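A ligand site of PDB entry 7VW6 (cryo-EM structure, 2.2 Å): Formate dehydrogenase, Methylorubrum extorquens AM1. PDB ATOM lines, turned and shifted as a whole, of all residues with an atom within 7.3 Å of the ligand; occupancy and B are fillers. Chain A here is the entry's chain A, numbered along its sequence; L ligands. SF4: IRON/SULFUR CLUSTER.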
ATOM      1  N   LEU A 101      -8.676 -21.315  10.276  1.00  0.00           N
ATOM      2  CA  LEU A 101      -7.644 -20.927   9.326  1.00  0.00           C
ATOM      3  C   LEU A 101      -8.090 -19.803   8.411  1.00  0.00           C
ATOM      4  O   LEU A 101      -7.396 -18.787   8.302  1.00  0.00           O
ATOM      5  CB  LEU A 101      -7.208 -22.138   8.486  1.00  0.00           C
ATOM      6  CG  LEU A 101      -6.536 -23.265   9.275  1.00  0.00           C
ATOM      7  CD1 LEU A 101      -6.259 -24.439   8.368  1.00  0.00           C
ATOM      8  CD2 LEU A 101      -5.272 -22.770   9.932  1.00  0.00           C
ATOM      9  N   CYS A 102      -9.235 -19.949   7.748  1.00  0.00           N
ATOM     10  CA  CYS A 102      -9.675 -18.950   6.777  1.00  0.00           C
ATOM     11  C   CYS A 102     -10.376 -17.763   7.419  1.00  0.00           C
ATOM     12  O   CYS A 102     -10.617 -16.766   6.724  1.00  0.00           O
ATOM     13  CB  CYS A 102     -10.584 -19.603   5.735  1.00  0.00           C
ATOM     14  SG  CYS A 102     -12.284 -19.869   6.261  1.00  0.00           S
ATOM     15  N   GLN A 164       1.979 -29.409   2.701  1.00  0.00           N
ATOM     16  CA  GLN A 164       2.874 -28.372   3.199  1.00  0.00           C
ATOM     17  C   GLN A 164       4.337 -28.787   3.024  1.00  0.00           C
ATOM     18  O   GLN A 164       4.663 -29.967   3.160  1.00  0.00           O
ATOM     19  CB  GLN A 164       2.599 -28.091   4.676  1.00  0.00           C
ATOM     20  CG  GLN A 164       1.314 -27.337   4.936  1.00  0.00           C
ATOM     21  CD  GLN A 164       1.409 -25.884   4.538  1.00  0.00           C
ATOM     22  OE1 GLN A 164       2.249 -25.141   5.044  1.00  0.00           O
ATOM     23  NE2 GLN A 164       0.547 -25.471   3.622  1.00  0.00           N
ATOM     24  N   VAL A 208       6.726 -14.673  -3.137  1.00  0.00           N
ATOM     25  CA  VAL A 208       5.574 -15.537  -3.350  1.00  0.00           C
ATOM     26  C   VAL A 208       6.077 -16.967  -3.460  1.00  0.00           C
ATOM     27  O   VAL A 208       6.924 -17.285  -4.303  1.00  0.00           O
ATOM     28  CB  VAL A 208       4.793 -15.130  -4.613  1.00  0.00           C
ATOM     29  CG1 VAL A 208       3.581 -16.027  -4.816  1.00  0.00           C
ATOM     30  CG2 VAL A 208       4.378 -13.674  -4.531  1.00  0.00           C
ATOM     31  N   ASN A 209       5.557 -17.841  -2.594  1.00  0.00           N
ATOM     32  CA  ASN A 209       5.901 -19.264  -2.580  1.00  0.00           C
ATOM     33  C   ASN A 209       4.591 -20.024  -2.361  1.00  0.00           C
ATOM     34  O   ASN A 209       4.218 -20.325  -1.229  1.00  0.00           O
ATOM     35  CB  ASN A 209       6.905 -19.584  -1.482  1.00  0.00           C
ATOM     36  CG  ASN A 209       8.301 -19.102  -1.807  1.00  0.00           C
ATOM     37  OD1 ASN A 209       9.002 -19.710  -2.606  1.00  0.00           O
ATOM     38  ND2 ASN A 209       8.698 -17.999  -1.194  1.00  0.00           N
ATOM     39  N   LEU A 210       3.913 -20.356  -3.464  1.00  0.00           N
ATOM     40  CA  LEU A 210       2.578 -20.914  -3.373  1.00  0.00           C
ATOM     41  C   LEU A 210       2.566 -22.418  -3.115  1.00  0.00           C
ATOM     42  O   LEU A 210       1.477 -23.000  -3.028  1.00  0.00           O
ATOM     43  CB  LEU A 210       1.775 -20.604  -4.637  1.00  0.00           C
ATOM     44  CG  LEU A 210       1.359 -19.147  -4.842  1.00  0.00           C
ATOM     45  CD1 LEU A 210       0.571 -18.995  -6.136  1.00  0.00           C
ATOM     46  CD2 LEU A 210       0.577 -18.601  -3.662  1.00  0.00           C
ATOM     47  N   ALA A 212       3.121 -23.544  -0.351  1.00  0.00           N
ATOM     48  CA  ALA A 212       2.575 -23.607   1.001  1.00  0.00           C
ATOM     49  C   ALA A 212       1.171 -23.000   1.094  1.00  0.00           C
ATOM     50  O   ALA A 212       0.665 -22.812   2.196  1.00  0.00           O
ATOM     51  CB  ALA A 212       3.510 -22.902   1.981  1.00  0.00           C
ATOM     52  N   CYS A 213       0.533 -22.704  -0.043  1.00  0.00           N
ATOM     53  CA  CYS A 213      -0.802 -22.137  -0.036  1.00  0.00           C
ATOM     54  C   CYS A 213      -1.840 -23.181   0.355  1.00  0.00           C
ATOM     55  O   CYS A 213      -1.746 -24.340  -0.037  1.00  0.00           O
ATOM     56  CB  CYS A 213      -1.133 -21.545  -1.410  1.00  0.00           C
ATOM     57  SG  CYS A 213      -2.754 -20.759  -1.526  1.00  0.00           S
ATOM     58  N   ILE A 214      -2.833 -22.764   1.141  1.00  0.00           N
ATOM     59  CA  ILE A 214      -3.958 -23.620   1.499  1.00  0.00           C
ATOM     60  C   ILE A 214      -5.261 -23.143   0.871  1.00  0.00           C
ATOM     61  O   ILE A 214      -6.325 -23.668   1.196  1.00  0.00           O
ATOM     62  CB  ILE A 214      -4.114 -23.749   3.028  1.00  0.00           C
ATOM     63  CG1 ILE A 214      -4.185 -22.371   3.685  1.00  0.00           C
ATOM     64  CG2 ILE A 214      -3.007 -24.603   3.611  1.00  0.00           C
ATOM     65  CD1 ILE A 214      -5.054 -22.332   4.913  1.00  0.00           C
ATOM     66  N   GLN A 215      -5.198 -22.154  -0.027  1.00  0.00           N
ATOM     67  CA  GLN A 215      -6.364 -21.646  -0.760  1.00  0.00           C
ATOM     68  C   GLN A 215      -7.463 -21.154   0.185  1.00  0.00           C
ATOM     69  O   GLN A 215      -8.647 -21.440  -0.006  1.00  0.00           O
ATOM     70  CB  GLN A 215      -6.911 -22.712  -1.717  1.00  0.00           C
ATOM     71  CG  GLN A 215      -6.067 -22.903  -2.974  1.00  0.00           C
ATOM     72  CD  GLN A 215      -5.469 -24.284  -3.075  1.00  0.00           C
ATOM     73  OE1 GLN A 215      -4.987 -24.838  -2.095  1.00  0.00           O
ATOM     74  NE2 GLN A 215      -5.478 -24.852  -4.277  1.00  0.00           N
ATOM     75  N   CYS A 216      -7.064 -20.385   1.197  1.00  0.00           N
ATOM     76  CA  CYS A 216      -8.027 -19.851   2.150  1.00  0.00           C
ATOM     77  C   CYS A 216      -8.737 -18.591   1.656  1.00  0.00           C
ATOM     78  O   CYS A 216      -9.765 -18.217   2.238  1.00  0.00           O
ATOM     79  CB  CYS A 216      -7.316 -19.542   3.474  1.00  0.00           C
ATOM     80  SG  CYS A 216      -6.149 -18.175   3.379  1.00  0.00           S
ATOM     81  N   ASN A 217      -8.231 -17.937   0.606  1.00  0.00           N
ATOM     82  CA  ASN A 217      -8.743 -16.699   0.017  1.00  0.00           C
ATOM     83  C   ASN A 217      -8.561 -15.472   0.903  1.00  0.00           C
ATOM     84  O   ASN A 217      -9.140 -14.427   0.603  1.00  0.00           O
ATOM     85  CB  ASN A 217     -10.226 -16.774  -0.366  1.00  0.00           C
ATOM     86  CG  ASN A 217     -10.610 -18.100  -0.992  1.00  0.00           C
ATOM     87  OD1 ASN A 217      -9.902 -18.610  -1.864  1.00  0.00           O
ATOM     88  ND2 ASN A 217     -11.741 -18.644  -0.578  1.00  0.00           N
ATOM     89  N   LEU A 218      -7.773 -15.549   1.976  1.00  0.00           N
ATOM     90  CA  LEU A 218      -7.587 -14.360   2.810  1.00  0.00           C
ATOM     91  C   LEU A 218      -6.868 -13.252   2.045  1.00  0.00           C
ATOM     92  O   LEU A 218      -7.166 -12.074   2.240  1.00  0.00           O
ATOM     93  CB  LEU A 218      -6.838 -14.721   4.094  1.00  0.00           C
ATOM     94  CG  LEU A 218      -7.719 -15.115   5.286  1.00  0.00           C
ATOM     95  CD1 LEU A 218      -6.886 -15.684   6.413  1.00  0.00           C
ATOM     96  CD2 LEU A 218      -8.558 -13.945   5.787  1.00  0.00           C
ATOM     97  N   CYS A 219      -5.918 -13.620   1.182  1.00  0.00           N
ATOM     98  CA  CYS A 219      -5.242 -12.608   0.366  1.00  0.00           C
ATOM     99  C   CYS A 219      -6.183 -11.989  -0.647  1.00  0.00           C
ATOM    100  O   CYS A 219      -6.096 -10.788  -0.934  1.00  0.00           O
ATOM    101  CB  CYS A 219      -4.043 -13.228  -0.337  1.00  0.00           C
ATOM    102  SG  CYS A 219      -4.452 -14.663  -1.340  1.00  0.00           S
ATOM    103  N   VAL A 220      -7.091 -12.789  -1.218  1.00  0.00           N
ATOM    104  CA  VAL A 220      -8.073 -12.256  -2.151  1.00  0.00           C
ATOM    105  C   VAL A 220      -8.958 -11.224  -1.458  1.00  0.00           C
ATOM    106  O   VAL A 220      -9.219 -10.137  -1.993  1.00  0.00           O
ATOM    107  CB  VAL A 220      -8.927 -13.383  -2.758  1.00  0.00           C
ATOM    108  CG1 VAL A 220     -10.049 -12.801  -3.595  1.00  0.00           C
ATOM    109  CG2 VAL A 220      -8.072 -14.321  -3.590  1.00  0.00           C
ATOM    110  N   ARG A 221      -9.442 -11.556  -0.265  1.00  0.00           N
ATOM    111  CA  ARG A 221     -10.229 -10.595   0.506  1.00  0.00           C
ATOM    112  C   ARG A 221      -9.404  -9.355   0.830  1.00  0.00           C
ATOM    113  O   ARG A 221      -9.881  -8.228   0.658  1.00  0.00           O
ATOM    114  CB  ARG A 221     -10.774 -11.247   1.774  1.00  0.00           C
ATOM    115  CG  ARG A 221     -12.090 -11.985   1.568  1.00  0.00           C
ATOM    116  CD  ARG A 221     -12.468 -12.864   2.753  1.00  0.00           C
ATOM    117  NE  ARG A 221     -11.668 -14.079   2.803  1.00  0.00           N
ATOM    118  CZ  ARG A 221     -11.488 -14.826   3.891  1.00  0.00           C
ATOM    119  NH1 ARG A 221     -12.023 -14.495   5.053  1.00  0.00           N
ATOM    120  NH2 ARG A 221     -10.738 -15.916   3.809  1.00  0.00           N
ATOM    121  N   ILE A 232      -5.275  -9.285  -7.035  1.00  0.00           N
ATOM    122  CA  ILE A 232      -5.262 -10.731  -6.828  1.00  0.00           C
ATOM    123  C   ILE A 232      -6.591 -11.328  -7.258  1.00  0.00           C
ATOM    124  O   ILE A 232      -7.657 -10.721  -7.092  1.00  0.00           O
ATOM    125  CB  ILE A 232      -4.942 -11.064  -5.355  1.00  0.00           C
ATOM    126  CG1 ILE A 232      -3.482 -10.723  -5.029  1.00  0.00           C
ATOM    127  CG2 ILE A 232      -5.233 -12.524  -5.029  1.00  0.00           C
ATOM    128  CD1 ILE A 232      -3.092 -11.055  -3.613  1.00  0.00           C
ATOM    129  N   MET A 234      -8.405 -15.625  -7.682  1.00  0.00           N
ATOM    130  CA  MET A 234      -8.274 -17.083  -7.640  1.00  0.00           C
ATOM    131  C   MET A 234      -8.784 -17.622  -8.971  1.00  0.00           C
ATOM    132  O   MET A 234      -9.974 -17.490  -9.269  1.00  0.00           O
ATOM    133  CB  MET A 234      -9.044 -17.679  -6.463  1.00  0.00           C
ATOM    134  CG  MET A 234      -8.757 -19.148  -6.217  1.00  0.00           C
ATOM    135  SD  MET A 234      -7.195 -19.452  -5.380  1.00  0.00           S
ATOM    136  CE  MET A 234      -7.436 -18.579  -3.841  1.00  0.00           C
ATOM    137  N   VAL A 243      -3.706 -18.728  -6.673  1.00  0.00           N
ATOM    138  CA  VAL A 243      -3.599 -17.287  -6.499  1.00  0.00           C
ATOM    139  C   VAL A 243      -2.836 -16.697  -7.682  1.00  0.00           C
ATOM    140  O   VAL A 243      -1.737 -17.165  -8.026  1.00  0.00           O
ATOM    141  CB  VAL A 243      -2.898 -16.956  -5.171  1.00  0.00           C
ATOM    142  CG1 VAL A 243      -2.611 -15.465  -5.059  1.00  0.00           C
ATOM    143  CG2 VAL A 243      -3.712 -17.459  -3.989  1.00  0.00           C
ATOM    144  N   CYS A 262      -2.042  -8.294   1.709  1.00  0.00           N
ATOM    145  CA  CYS A 262      -2.108  -9.741   1.534  1.00  0.00           C
ATOM    146  C   CYS A 262      -1.054 -10.456   2.368  1.00  0.00           C
ATOM    147  O   CYS A 262      -1.317 -11.509   2.937  1.00  0.00           O
ATOM    148  CB  CYS A 262      -1.963 -10.101   0.045  1.00  0.00           C
ATOM    149  SG  CYS A 262      -0.516  -9.400  -0.775  1.00  0.00           S
ATOM    150  N   VAL A 263       0.151  -9.870   2.457  1.00  0.00           N
ATOM    151  CA  VAL A 263       1.211 -10.456   3.274  1.00  0.00           C
ATOM    152  C   VAL A 263       0.786 -10.524   4.737  1.00  0.00           C
ATOM    153  O   VAL A 263       0.957 -11.544   5.404  1.00  0.00           O
ATOM    154  CB  VAL A 263       2.517  -9.657   3.106  1.00  0.00           C
ATOM    155  CG1 VAL A 263       3.557 -10.125   4.108  1.00  0.00           C
ATOM    156  CG2 VAL A 263       3.034  -9.784   1.680  1.00  0.00           C
ATOM    157  N   ALA A 265      -2.231 -10.610   5.850  1.00  0.00           N
ATOM    158  CA  ALA A 265      -3.363 -11.520   6.004  1.00  0.00           C
ATOM    159  C   ALA A 265      -2.970 -12.994   5.929  1.00  0.00           C
ATOM    160  O   ALA A 265      -3.605 -13.827   6.587  1.00  0.00           O
ATOM    161  CB  ALA A 265      -4.430 -11.208   4.943  1.00  0.00           C
ATOM    162  N   CYS A 266      -1.950 -13.344   5.151  1.00  0.00           N
ATOM    163  CA  CYS A 266      -1.699 -14.740   4.824  1.00  0.00           C
ATOM    164  C   CYS A 266      -1.281 -15.541   6.058  1.00  0.00           C
ATOM    165  O   CYS A 266      -0.363 -15.128   6.770  1.00  0.00           O
ATOM    166  CB  CYS A 266      -0.614 -14.853   3.750  1.00  0.00           C
ATOM    167  SG  CYS A 266      -0.247 -16.545   3.234  1.00  0.00           S
ATOM    168  N   PRO A 267      -1.908 -16.681   6.332  1.00  0.00           N
ATOM    169  CA  PRO A 267      -1.594 -17.464   7.530  1.00  0.00           C
ATOM    170  C   PRO A 267      -0.566 -18.582   7.364  1.00  0.00           C
ATOM    171  O   PRO A 267      -0.260 -19.247   8.359  1.00  0.00           O
ATOM    172  CB  PRO A 267      -2.961 -18.068   7.880  1.00  0.00           C
ATOM    173  CG  PRO A 267      -3.624 -18.269   6.554  1.00  0.00           C
ATOM    174  CD  PRO A 267      -3.061 -17.243   5.592  1.00  0.00           C
ATOM    175  N   THR A 268      -0.032 -18.824   6.164  1.00  0.00           N
ATOM    176  CA  THR A 268       0.832 -19.969   5.931  1.00  0.00           C
ATOM    177  C   THR A 268       2.279 -19.625   5.626  1.00  0.00           C
ATOM    178  O   THR A 268       3.132 -20.519   5.679  1.00  0.00           O
ATOM    179  CB  THR A 268       0.289 -20.834   4.778  1.00  0.00           C
ATOM    180  OG1 THR A 268       0.118 -20.017   3.608  1.00  0.00           O
ATOM    181  CG2 THR A 268      -1.033 -21.467   5.147  1.00  0.00           C
ATOM    182  N   GLY A 269       2.587 -18.376   5.305  1.00  0.00           N
ATOM    183  CA  GLY A 269       3.901 -18.033   4.819  1.00  0.00           C
ATOM    184  C   GLY A 269       4.079 -18.155   3.332  1.00  0.00           C
ATOM    185  O   GLY A 269       5.189 -17.938   2.834  1.00  0.00           O
ATOM    186  N   ALA A 270       3.015 -18.501   2.596  1.00  0.00           N
ATOM    187  CA  ALA A 270       3.082 -18.472   1.140  1.00  0.00           C
ATOM    188  C   ALA A 270       3.454 -17.088   0.630  1.00  0.00           C
ATOM    189  O   ALA A 270       4.145 -16.953  -0.378  1.00  0.00           O
ATOM    190  CB  ALA A 270       1.752 -18.940   0.542  1.00  0.00           C
ATOM    191  N   LEU A 271       2.994 -16.048   1.315  1.00  0.00           N
ATOM    192  CA  LEU A 271       3.370 -14.669   1.039  1.00  0.00           C
ATOM    193  C   LEU A 271       4.093 -14.117   2.257  1.00  0.00           C
ATOM    194  O   LEU A 271       3.563 -14.169   3.367  1.00  0.00           O
ATOM    195  CB  LEU A 271       2.148 -13.811   0.696  1.00  0.00           C
ATOM    196  CG  LEU A 271       1.157 -14.383  -0.309  1.00  0.00           C
ATOM    197  CD1 LEU A 271      -0.142 -13.610  -0.250  1.00  0.00           C
ATOM    198  CD2 LEU A 271       1.727 -14.334  -1.707  1.00  0.00           C
HETATM  199 FE1  SF4 L   1      -3.654 -16.404  -0.118  1.00  0.00          FE
HETATM  200 FE2  SF4 L   1      -4.446 -18.131   1.867  1.00  0.00          FE
HETATM  201 FE3  SF4 L   1      -1.861 -17.209   1.783  1.00  0.00          FE
HETATM  202 FE4  SF4 L   1      -2.749 -18.980  -0.117  1.00  0.00          FE
HETATM  203  S1  SF4 L   1      -2.551 -19.364   2.125  1.00  0.00           S
HETATM  204  S2  SF4 L   1      -1.514 -17.094  -0.467  1.00  0.00           S
HETATM  205  S3  SF4 L   1      -4.910 -18.296  -0.363  1.00  0.00           S
HETATM  206  S4  SF4 L   1      -3.735 -15.970   2.121  1.00  0.00           S
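The backbone NH (N) of Leu 218 sits close to the side-chain sulfur (SG) of Cys 216, at 3.4 Å. SG of Cys 213 sits close to N of Gln 215 (3.2 Å). The side-chain hydroxyl (OG1) of Thr 268 lies close to the side-chain sulfur (SG) of Cys 266, 3.5 Å away. The backbone carbonyl oxygen of Ala 270 sits at hydrogen-bond distance from the backbone NH of Asn 209 (2.8 Å). The side-chain sulfur of Met 234 sits at hydrogen-bond distance from the backbone NH of Val 243, 3.8 Å away. N of Leu 271 sits close to SG of Cys 266 (3.8 Å). The backbone carbonyl oxygen (O) of Cys 216 lies within hydrogen-bond range of the guanidinium group (NH2) of Arg 221 (3.0 Å). The side-chain hydroxyl of Thr 268 is in hydrogen-bond range of the backbone carbonyl oxygen of Ala 212 (3.2 Å).
Gln 215 touches the ligand. CB of Leu 218 touches S4 of the ligand (3.9 Å). Val 243 touches the ligand (CG2 to S3, 3.9 Å). Pro 267 touches the ligand. Ala 270 touches the ligand (CB to S2, 3.9 Å). CD1 of Leu 271 touches S2 of the ligand (3.8 Å). Hydrophobic or aromatic side chains that line the ligand: Ile 214, Leu 218, Val 243, Pro 267, Ala 270 and Leu 271.
S4 of the ligand lies close to N of Cys 219 (3.3 Å). N of Ile 214 sits close to S1 of the ligand. SG of Cys 216 binds FE2 of the ligand (2.3 Å). OG1 of Thr 268 lies close to S1 of the ligand (3.1 Å). FE3 of the ligand is bound by SG of Cys 266 (2.3 Å). The side-chain sulfur (SG) of Cys 219 is bound to an iron atom (FE1) of the ligand (2.3 Å). SG of Cys 213 binds FE4 of the ligand, at 2.3 Å. A sulfur (S3) of the ligand sits close to the backbone NH (N) of Cys 216 (3.4 Å). N of Asn 217 sits close to S3 of the ligand (3.5 Å).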
